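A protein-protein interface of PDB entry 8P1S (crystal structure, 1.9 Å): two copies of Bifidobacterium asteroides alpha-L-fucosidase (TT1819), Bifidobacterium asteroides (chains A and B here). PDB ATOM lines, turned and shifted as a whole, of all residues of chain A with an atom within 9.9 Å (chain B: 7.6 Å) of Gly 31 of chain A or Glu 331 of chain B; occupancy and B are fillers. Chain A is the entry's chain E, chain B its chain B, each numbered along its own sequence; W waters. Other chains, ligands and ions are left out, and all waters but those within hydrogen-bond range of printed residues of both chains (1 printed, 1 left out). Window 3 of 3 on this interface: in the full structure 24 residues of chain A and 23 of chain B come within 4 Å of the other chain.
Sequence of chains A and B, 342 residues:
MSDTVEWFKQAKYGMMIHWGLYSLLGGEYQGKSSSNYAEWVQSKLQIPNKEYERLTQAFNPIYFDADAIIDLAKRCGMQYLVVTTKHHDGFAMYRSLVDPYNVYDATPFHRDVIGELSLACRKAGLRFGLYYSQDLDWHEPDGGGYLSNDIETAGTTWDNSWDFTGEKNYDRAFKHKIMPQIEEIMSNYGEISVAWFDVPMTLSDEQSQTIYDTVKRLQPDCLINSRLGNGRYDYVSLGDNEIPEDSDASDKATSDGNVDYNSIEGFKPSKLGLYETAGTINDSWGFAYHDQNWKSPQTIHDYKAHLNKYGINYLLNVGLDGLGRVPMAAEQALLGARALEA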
ATOM      1  N   LEU A  25      16.648   5.389   5.731  1.00  0.00           N
ATOM      2  CA  LEU A  25      17.737   4.970   4.842  1.00  0.00           C
ATOM      3  C   LEU A  25      17.415   3.643   4.170  1.00  0.00           C
ATOM      4  O   LEU A  25      17.790   3.390   3.030  1.00  0.00           O
ATOM      5  CB  LEU A  25      19.016   4.862   5.644  1.00  0.00           C
ATOM      6  CG  LEU A  25      19.632   6.171   6.121  1.00  0.00           C
ATOM      7  CD1 LEU A  25      20.868   5.886   6.937  1.00  0.00           C
ATOM      8  CD2 LEU A  25      20.019   7.070   4.960  1.00  0.00           C
ATOM      9  N   GLY A  27      18.343   0.587   4.437  1.00  0.00           N
ATOM     10  CA  GLY A  27      19.333  -0.415   4.064  1.00  0.00           C
ATOM     11  C   GLY A  27      20.450   0.109   3.180  1.00  0.00           C
ATOM     12  O   GLY A  27      21.272  -0.691   2.748  1.00  0.00           O
ATOM     13  N   GLU A  28      20.442   1.416   2.854  1.00  0.00           N
ATOM     14  CA  GLU A  28      21.505   1.922   2.006  1.00  0.00           C
ATOM     15  C   GLU A  28      21.870   3.347   2.445  1.00  0.00           C
ATOM     16  O   GLU A  28      21.060   4.106   2.948  1.00  0.00           O
ATOM     17  CB  GLU A  28      21.159   1.730   0.512  1.00  0.00           C
ATOM     18  CG  GLU A  28      19.903   2.387   0.033  1.00  0.00           C
ATOM     19  CD  GLU A  28      19.620   2.171  -1.450  1.00  0.00           C
ATOM     20  OE1 GLU A  28      19.225   1.040  -1.744  1.00  0.00           O
ATOM     21  OE2 GLU A  28      19.916   3.122  -2.294  1.00  0.00           O
ATOM     22  N   TYR A  29      23.106   3.713   2.172  1.00  0.00           N
ATOM     23  CA  TYR A  29      23.599   5.059   2.482  1.00  0.00           C
ATOM     24  C   TYR A  29      24.762   5.366   1.572  1.00  0.00           C
ATOM     25  O   TYR A  29      25.642   4.522   1.410  1.00  0.00           O
ATOM     26  CB  TYR A  29      24.061   5.134   3.927  1.00  0.00           C
ATOM     27  CG  TYR A  29      24.678   6.455   4.315  1.00  0.00           C
ATOM     28  CD1 TYR A  29      23.880   7.537   4.624  1.00  0.00           C
ATOM     29  CD2 TYR A  29      26.063   6.631   4.369  1.00  0.00           C
ATOM     30  CE1 TYR A  29      24.423   8.774   4.961  1.00  0.00           C
ATOM     31  CE2 TYR A  29      26.626   7.847   4.763  1.00  0.00           C
ATOM     32  CZ  TYR A  29      25.790   8.919   5.051  1.00  0.00           C
ATOM     33  OH  TYR A  29      26.219  10.137   5.435  1.00  0.00           O
ATOM     34  N   GLN A  30      24.608   6.455   0.821  1.00  0.00           N
ATOM     35  CA  GLN A  30      25.581   6.940  -0.142  1.00  0.00           C
ATOM     36  C   GLN A  30      26.070   5.828  -1.056  1.00  0.00           C
ATOM     37  O   GLN A  30      27.253   5.676  -1.307  1.00  0.00           O
ATOM     38  CB  GLN A  30      26.780   7.520   0.587  1.00  0.00           C
ATOM     39  CG  GLN A  30      26.521   8.828   1.331  1.00  0.00           C
ATOM     40  CD  GLN A  30      27.794   9.330   2.032  1.00  0.00           C
ATOM     41  OE1 GLN A  30      28.829   8.651   2.235  1.00  0.00           O
ATOM     42  NE2 GLN A  30      27.722  10.579   2.480  1.00  0.00           N
ATOM     43  N   GLY A  31      25.147   5.068  -1.587  1.00  0.00           N
ATOM     44  CA  GLY A  31      25.486   4.096  -2.600  1.00  0.00           C
ATOM     45  C   GLY A  31      26.065   2.784  -2.034  1.00  0.00           C
ATOM     46  O   GLY A  31      26.409   1.952  -2.797  1.00  0.00           O
ATOM     47  N   LYS A  32      26.103   2.607  -0.710  1.00  0.00           N
ATOM     48  CA  LYS A  32      26.587   1.398  -0.057  1.00  0.00           C
ATOM     49  C   LYS A  32      25.471   0.779   0.788  1.00  0.00           C
ATOM     50  O   LYS A  32      24.534   1.427   1.265  1.00  0.00           O
ATOM     51  CB  LYS A  32      27.801   1.740   0.816  1.00  0.00           C
ATOM     52  CG  LYS A  32      28.993   2.279   0.029  1.00  0.00           C
ATOM     53  CD  LYS A  32      30.134   2.746   0.960  1.00  0.00           C
ATOM     54  CE  LYS A  32      31.482   3.031   0.306  1.00  0.00           C
ATOM     55  NZ  LYS A  32      31.675   2.403  -1.030  1.00  0.00           N
ATOM     56  N   SER A  33      25.614  -0.496   0.975  1.00  0.00           N
ATOM     57  CA  SER A  33      24.616  -1.362   1.575  1.00  0.00           C
ATOM     58  C   SER A  33      24.854  -1.588   3.075  1.00  0.00           C
ATOM     59  O   SER A  33      25.999  -1.804   3.471  1.00  0.00           O
ATOM     60  CB  SER A  33      24.722  -2.681   0.834  1.00  0.00           C
ATOM     61  OG  SER A  33      23.682  -3.446   1.344  1.00  0.00           O
ATOM     62  N   SER A  34      23.781  -1.609   3.871  1.00  0.00           N
ATOM     63  CA  SER A  34      23.781  -2.297   5.158  1.00  0.00           C
ATOM     64  C   SER A  34      23.907  -3.818   4.927  1.00  0.00           C
ATOM     65  O   SER A  34      23.782  -4.306   3.806  1.00  0.00           O
ATOM     66  CB  SER A  34      22.475  -2.081   5.865  1.00  0.00           C
ATOM     67  OG  SER A  34      21.522  -3.025   5.331  1.00  0.00           O
ATOM     68  N   VAL A  41      22.848  -0.013   9.975  1.00  0.00           N
ATOM     69  CA  VAL A  41      23.523   0.733   8.923  1.00  0.00           C
ATOM     70  C   VAL A  41      24.513   1.753   9.499  1.00  0.00           C
ATOM     71  O   VAL A  41      25.588   1.979   8.918  1.00  0.00           O
ATOM     72  CB  VAL A  41      22.521   1.396   7.943  1.00  0.00           C
ATOM     73  CG1 VAL A  41      21.773   2.623   8.603  1.00  0.00           C
ATOM     74  CG2 VAL A  41      23.256   1.744   6.668  1.00  0.00           C
ATOM     75  N   LEU A  45      28.331   1.254   8.106  1.00  0.00           N
ATOM     76  CA  LEU A  45      29.011   2.197   7.224  1.00  0.00           C
ATOM     77  C   LEU A  45      29.659   3.328   8.016  1.00  0.00           C
ATOM     78  O   LEU A  45      30.102   4.280   7.413  1.00  0.00           O
ATOM     79  CB  LEU A  45      27.990   2.722   6.201  1.00  0.00           C
ATOM     80  CG  LEU A  45      27.379   1.629   5.350  1.00  0.00           C
ATOM     81  CD1 LEU A  45      26.249   2.160   4.462  1.00  0.00           C
ATOM     82  CD2 LEU A  45      28.460   0.899   4.511  1.00  0.00           C
ATOM     83  N   ILE A  47      28.682   5.863   9.911  1.00  0.00           N
ATOM     84  CA  ILE A  47      28.092   7.144   9.571  1.00  0.00           C
ATOM     85  C   ILE A  47      28.333   8.056  10.765  1.00  0.00           C
ATOM     86  O   ILE A  47      27.868   7.789  11.853  1.00  0.00           O
ATOM     87  CB  ILE A  47      26.599   7.005   9.194  1.00  0.00           C
ATOM     88  CG1 ILE A  47      26.376   5.961   8.104  1.00  0.00           C
ATOM     89  CG2 ILE A  47      26.010   8.366   8.791  1.00  0.00           C
ATOM     90  CD1 ILE A  47      24.935   5.692   7.835  1.00  0.00           C
ATOM     91  N   ALA B  68      25.926  15.262  -8.213  1.00  0.00           N
ATOM     92  CA  ALA B  68      26.341  13.875  -8.043  1.00  0.00           C
ATOM     93  C   ALA B  68      25.607  13.011  -9.052  1.00  0.00           C
ATOM     94  O   ALA B  68      26.185  12.093  -9.638  1.00  0.00           O
ATOM     95  CB  ALA B  68      26.175  13.359  -6.602  1.00  0.00           C
ATOM     96  N   LEU B  72      27.439  10.826 -12.108  1.00  0.00           N
ATOM     97  CA  LEU B  72      27.209   9.422 -12.402  1.00  0.00           C
ATOM     98  C   LEU B  72      26.918   9.223 -13.884  1.00  0.00           C
ATOM     99  O   LEU B  72      27.531   8.373 -14.556  1.00  0.00           O
ATOM    100  CB  LEU B  72      26.079   8.876 -11.501  1.00  0.00           C
ATOM    101  CG  LEU B  72      25.643   7.456 -11.822  1.00  0.00           C
ATOM    102  CD1 LEU B  72      26.798   6.449 -11.617  1.00  0.00           C
ATOM    103  CD2 LEU B  72      24.420   7.118 -10.991  1.00  0.00           C
ATOM    104  N   ARG B  75      30.086   9.699 -15.907  1.00  0.00           N
ATOM    105  CA  ARG B  75      31.061   8.626 -15.807  1.00  0.00           C
ATOM    106  C   ARG B  75      30.613   7.412 -16.605  1.00  0.00           C
ATOM    107  O   ARG B  75      31.461   6.638 -17.056  1.00  0.00           O
ATOM    108  CB  ARG B  75      31.284   8.257 -14.338  1.00  0.00           C
ATOM    109  CG  ARG B  75      32.328   9.179 -13.719  1.00  0.00           C
ATOM    110  CD  ARG B  75      32.808   8.734 -12.354  1.00  0.00           C
ATOM    111  NE  ARG B  75      31.781   9.080 -11.411  1.00  0.00           N
ATOM    112  CZ  ARG B  75      31.059   8.220 -10.694  1.00  0.00           C
ATOM    113  NH1 ARG B  75      31.458   6.985 -10.518  1.00  0.00           N
ATOM    114  NH2 ARG B  75      29.953   8.620 -10.100  1.00  0.00           N
ATOM    115  N   CYS B  76      29.293   7.216 -16.764  1.00  0.00           N
ATOM    116  CA  CYS B  76      28.784   6.082 -17.545  1.00  0.00           C
ATOM    117  C   CYS B  76      28.777   6.374 -19.061  1.00  0.00           C
ATOM    118  O   CYS B  76      28.424   5.533 -19.867  1.00  0.00           O
ATOM    119  CB  CYS B  76      27.409   5.683 -17.054  1.00  0.00           C
ATOM    120  SG  CYS B  76      27.454   5.057 -15.336  1.00  0.00           S
ATOM    121  N   ILE B 281      15.859   0.295 -15.575  1.00  0.00           N
ATOM    122  CA  ILE B 281      16.864  -0.590 -15.063  1.00  0.00           C
ATOM    123  C   ILE B 281      16.176  -1.752 -14.382  1.00  0.00           C
ATOM    124  O   ILE B 281      16.546  -2.906 -14.642  1.00  0.00           O
ATOM    125  CB  ILE B 281      17.903   0.107 -14.155  1.00  0.00           C
ATOM    126  CG1 ILE B 281      18.527   1.313 -14.821  1.00  0.00           C
ATOM    127  CG2 ILE B 281      18.989  -0.906 -13.767  1.00  0.00           C
ATOM    128  CD1 ILE B 281      19.318   2.226 -13.856  1.00  0.00           C
ATOM    129  N   TRP B 294      16.421  -5.781 -11.011  1.00  0.00           N
ATOM    130  CA  TRP B 294      17.382  -4.894 -11.640  1.00  0.00           C
ATOM    131  C   TRP B 294      18.103  -5.653 -12.750  1.00  0.00           C
ATOM    132  O   TRP B 294      18.659  -6.687 -12.496  1.00  0.00           O
ATOM    133  CB  TRP B 294      18.404  -4.411 -10.597  1.00  0.00           C
ATOM    134  CG  TRP B 294      17.794  -3.629  -9.480  1.00  0.00           C
ATOM    135  CD1 TRP B 294      17.610  -4.100  -8.215  1.00  0.00           C
ATOM    136  CD2 TRP B 294      17.325  -2.268  -9.473  1.00  0.00           C
ATOM    137  NE1 TRP B 294      17.018  -3.122  -7.445  1.00  0.00           N
ATOM    138  CE2 TRP B 294      16.816  -2.007  -8.187  1.00  0.00           C
ATOM    139  CE3 TRP B 294      17.261  -1.250 -10.418  1.00  0.00           C
ATOM    140  CZ2 TRP B 294      16.278  -0.776  -7.810  1.00  0.00           C
ATOM    141  CZ3 TRP B 294      16.740  -0.026 -10.057  1.00  0.00           C
ATOM    142  CH2 TRP B 294      16.254   0.208  -8.768  1.00  0.00           C
ATOM    143  N   VAL B 318      16.376   6.290 -14.359  1.00  0.00           N
ATOM    144  CA  VAL B 318      16.520   6.146 -12.924  1.00  0.00           C
ATOM    145  C   VAL B 318      15.302   6.803 -12.249  1.00  0.00           C
ATOM    146  O   VAL B 318      14.906   7.920 -12.549  1.00  0.00           O
ATOM    147  CB  VAL B 318      17.829   6.832 -12.468  1.00  0.00           C
ATOM    148  CG1 VAL B 318      17.898   7.030 -10.980  1.00  0.00           C
ATOM    149  CG2 VAL B 318      19.042   6.082 -12.945  1.00  0.00           C
ATOM    150  N   ARG B 325      17.631  10.040  -3.919  1.00  0.00           N
ATOM    151  CA  ARG B 325      18.784   9.203  -4.229  1.00  0.00           C
ATOM    152  C   ARG B 325      18.557   8.379  -5.465  1.00  0.00           C
ATOM    153  O   ARG B 325      17.483   7.849  -5.687  1.00  0.00           O
ATOM    154  CB  ARG B 325      19.138   8.243  -3.074  1.00  0.00           C
ATOM    155  CG  ARG B 325      19.316   8.903  -1.727  1.00  0.00           C
ATOM    156  CD  ARG B 325      19.760   7.967  -0.634  1.00  0.00           C
ATOM    157  NE  ARG B 325      18.637   7.082  -0.307  1.00  0.00           N
ATOM    158  CZ  ARG B 325      18.706   6.126   0.629  1.00  0.00           C
ATOM    159  NH1 ARG B 325      19.743   6.101   1.424  1.00  0.00           N
ATOM    160  NH2 ARG B 325      17.780   5.196   0.781  1.00  0.00           N
ATOM    161  N   VAL B 326      19.657   8.119  -6.165  1.00  0.00           N
ATOM    162  CA  VAL B 326      19.743   7.025  -7.114  1.00  0.00           C
ATOM    163  C   VAL B 326      19.803   5.778  -6.284  1.00  0.00           C
ATOM    164  O   VAL B 326      20.667   5.630  -5.465  1.00  0.00           O
ATOM    165  CB  VAL B 326      20.971   7.155  -8.026  1.00  0.00           C
ATOM    166  CG1 VAL B 326      21.175   5.943  -8.900  1.00  0.00           C
ATOM    167  CG2 VAL B 326      21.030   8.454  -8.821  1.00  0.00           C
ATOM    168  N   PRO B 327      18.887   4.807  -6.446  1.00  0.00           N
ATOM    169  CA  PRO B 327      18.982   3.577  -5.717  1.00  0.00           C
ATOM    170  C   PRO B 327      20.355   2.985  -5.942  1.00  0.00           C
ATOM    171  O   PRO B 327      20.850   3.004  -7.030  1.00  0.00           O
ATOM    172  CB  PRO B 327      17.855   2.719  -6.263  1.00  0.00           C
ATOM    173  CG  PRO B 327      16.839   3.763  -6.662  1.00  0.00           C
ATOM    174  CD  PRO B 327      17.682   4.864  -7.310  1.00  0.00           C
ATOM    175  N   MET B 328      20.928   2.430  -4.872  1.00  0.00           N
ATOM    176  CA  MET B 328      22.199   1.799  -4.882  1.00  0.00           C
ATOM    177  C   MET B 328      22.253   0.739  -5.983  1.00  0.00           C
ATOM    178  O   MET B 328      23.286   0.612  -6.648  1.00  0.00           O
ATOM    179  CB  MET B 328      22.454   1.141  -3.514  1.00  0.00           C
ATOM    180  CG  MET B 328      23.727   0.260  -3.518  1.00  0.00           C
ATOM    181  SD  MET B 328      24.003  -0.671  -2.019  1.00  0.00           S
ATOM    182  CE  MET B 328      22.347  -1.330  -1.726  1.00  0.00           C
ATOM    183  N   ALA B 329      21.221  -0.096  -6.118  1.00  0.00           N
ATOM    184  CA  ALA B 329      21.326  -1.178  -7.117  1.00  0.00           C
ATOM    185  C   ALA B 329      21.321  -0.588  -8.536  1.00  0.00           C
ATOM    186  O   ALA B 329      21.903  -1.135  -9.438  1.00  0.00           O
ATOM    187  CB  ALA B 329      20.204  -2.163  -6.946  1.00  0.00           C
ATOM    188  N   ALA B 330      20.755   0.598  -8.734  1.00  0.00           N
ATOM    189  CA  ALA B 330      20.715   1.218 -10.059  1.00  0.00           C
ATOM    190  C   ALA B 330      22.102   1.740 -10.377  1.00  0.00           C
ATOM    191  O   ALA B 330      22.624   1.469 -11.441  1.00  0.00           O
ATOM    192  CB  ALA B 330      19.659   2.283 -10.072  1.00  0.00           C
ATOM    193  N   GLU B 331      22.706   2.418  -9.400  1.00  0.00           N
ATOM    194  CA  GLU B 331      24.040   2.953  -9.532  1.00  0.00           C
ATOM    195  C   GLU B 331      25.026   1.831  -9.813  1.00  0.00           C
ATOM    196  O   GLU B 331      25.875   1.969 -10.696  1.00  0.00           O
ATOM    197  CB  GLU B 331      24.424   3.677  -8.235  1.00  0.00           C
ATOM    198  CG  GLU B 331      25.813   4.219  -8.212  1.00  0.00           C
ATOM    199  CD  GLU B 331      26.109   5.165  -7.065  1.00  0.00           C
ATOM    200  OE1 GLU B 331      25.338   5.303  -6.080  1.00  0.00           O
ATOM    201  OE2 GLU B 331      27.085   5.772  -7.162  1.00  0.00           O
ATOM    202  N   GLN B 332      24.918   0.740  -9.066  1.00  0.00           N
ATOM    203  CA  GLN B 332      25.803  -0.409  -9.249  1.00  0.00           C
ATOM    204  C   GLN B 332      25.617  -1.003 -10.635  1.00  0.00           C
ATOM    205  O   GLN B 332      26.592  -1.392 -11.262  1.00  0.00           O
ATOM    206  CB  GLN B 332      25.570  -1.510  -8.191  1.00  0.00           C
ATOM    207  CG  GLN B 332      26.036  -1.138  -6.783  1.00  0.00           C
ATOM    208  CD  GLN B 332      27.484  -0.695  -6.809  1.00  0.00           C
ATOM    209  OE1 GLN B 332      27.829   0.492  -6.654  1.00  0.00           O
ATOM    210  NE2 GLN B 332      28.365  -1.644  -7.093  1.00  0.00           N
ATOM    211  N   ALA B 333      24.371  -1.120 -11.117  1.00  0.00           N
ATOM    212  CA  ALA B 333      24.131  -1.682 -12.452  1.00  0.00           C
ATOM    213  C   ALA B 333      24.767  -0.787 -13.525  1.00  0.00           C
ATOM    214  O   ALA B 333      25.436  -1.256 -14.439  1.00  0.00           O
ATOM    215  CB  ALA B 333      22.646  -1.885 -12.672  1.00  0.00           C
ATOM    216  N   LEU B 334      24.597   0.507 -13.396  1.00  0.00           N
ATOM    217  CA  LEU B 334      25.106   1.451 -14.371  1.00  0.00           C
ATOM    218  C   LEU B 334      26.624   1.456 -14.370  1.00  0.00           C
ATOM    219  O   LEU B 334      27.224   1.470 -15.458  1.00  0.00           O
ATOM    220  CB  LEU B 334      24.583   2.847 -14.075  1.00  0.00           C
ATOM    221  CG  LEU B 334      23.083   3.056 -14.232  1.00  0.00           C
ATOM    222  CD1 LEU B 334      22.681   4.440 -13.704  1.00  0.00           C
ATOM    223  CD2 LEU B 334      22.686   2.937 -15.701  1.00  0.00           C
ATOM    224  N   LEU B 335      27.257   1.430 -13.162  1.00  0.00           N
ATOM    225  CA  LEU B 335      28.697   1.510 -13.118  1.00  0.00           C
ATOM    226  C   LEU B 335      29.301   0.182 -13.601  1.00  0.00           C
ATOM    227  O   LEU B 335      30.390   0.154 -14.174  1.00  0.00           O
ATOM    228  CB  LEU B 335      29.188   1.844 -11.715  1.00  0.00           C
ATOM    229  CG  LEU B 335      28.891   3.246 -11.211  1.00  0.00           C
ATOM    230  CD1 LEU B 335      29.175   3.352  -9.684  1.00  0.00           C
ATOM    231  CD2 LEU B 335      29.684   4.247 -12.009  1.00  0.00           C
ATOM    232  N   GLY B 336      28.581  -0.908 -13.376  1.00  0.00           N
ATOM    233  CA  GLY B 336      28.982  -2.214 -13.870  1.00  0.00           C
ATOM    234  C   GLY B 336      28.946  -2.295 -15.403  1.00  0.00           C
ATOM    235  O   GLY B 336      29.851  -2.855 -16.007  1.00  0.00           O
ATOM    236  N   ALA B 337      27.872  -1.780 -16.023  1.00  0.00           N
ATOM    237  CA  ALA B 337      27.787  -1.708 -17.487  1.00  0.00           C
ATOM    238  C   ALA B 337      28.946  -0.873 -18.064  1.00  0.00           C
ATOM    239  O   ALA B 337      29.609  -1.322 -19.015  1.00  0.00           O
ATOM    240  CB  ALA B 337      26.465  -1.157 -17.916  1.00  0.00           C
HETATM  241  O   HOH W   1      19.116  -0.281  -4.158  1.00  0.00           O
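NH2 of Arg 325 of chain B sits at hydrogen-bond distance from O of Leu 25 of chain A, at 2.9 Å. The guanidinium group of Arg 325 of chain B is in hydrogen-bond range of the backbone carbonyl oxygen of Glu 28 of chain A (2.8 Å). The backbone NH (N) of Met 328 of chain B sits at hydrogen-bond distance from the side-chain carboxylate (OE2) of Glu 28 of chain A. SD of Met 328 of chain B is in hydrogen-bond range of N of Ser 33 of chain A, 3.4 Å away. The backbone carbonyl oxygen (O) of Gly 31 of chain A sits close to the side-chain sulfur (SD) of Met 328 of chain B (3.6 Å).
Among the printed residues, merely in contact across the chains: Glu 28 of chain A with Pro 327 of chain B, Gly 31 of chain A with Glu 331 of chain B and Lys 32 of chain A with Met 328 of chain B.
Gln 30 of chain A touches none of the printed residues of chain B. Printed residues of chain B within 4 Å of Gly 31 of chain A: Met 328 and Glu 331. Of the printed residues of chain A, Arg 325 of chain B touches Leu 25 and Glu 28. Of the printed residues of chain A, Pro 327 of chain B touches Glu 28. Of chain A, only Glu 28, Gly 31, Lys 32 and Ser 33 come within 4 Å of Met 328 of chain B. No residue of chain A comes within 4 Å of Ala 329 of chain B. No residue of chain A comes within 4 Å of Ala 330 of chain B. Glu 331 of chain B touches just one residue of chain A: Gly 31 (3.7 Å). No residue of chain A comes within 4 Å of Gln 332 of chain B. The nearest residue of chain B that does not touch Gly 31 of chain A is Gln 332 of chain B (4.4 Å).
Of the 20 printed residues of chain B, 4 touch a printed residue of chain A. Hydrophobic or aromatic side chains of chain B that line the printed part of chain A: Met 328. Of the 12 printed residues of chain A, 5 touch a printed residue of chain B. Along chain A the printed residues that touch a printed residue of chain B span positions 25 to 33. Among the printed residues, no Asp or Glu carboxylate lies within 4 Å of a Lys or Arg side-chain nitrogen of the other chain.
No position is printed for both chains. Of the 8 pairs that touch across the chains among the printed residues, none has its exchanged pair printed and touching as well.
Water W1 lies within hydrogen-bond range of the side-chain carboxylate (OE1) of Glu 28 of chain A, the backbone NH (N) of Ala 329 of chain B and the backbone NH (N) of Met 328 of chain B.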
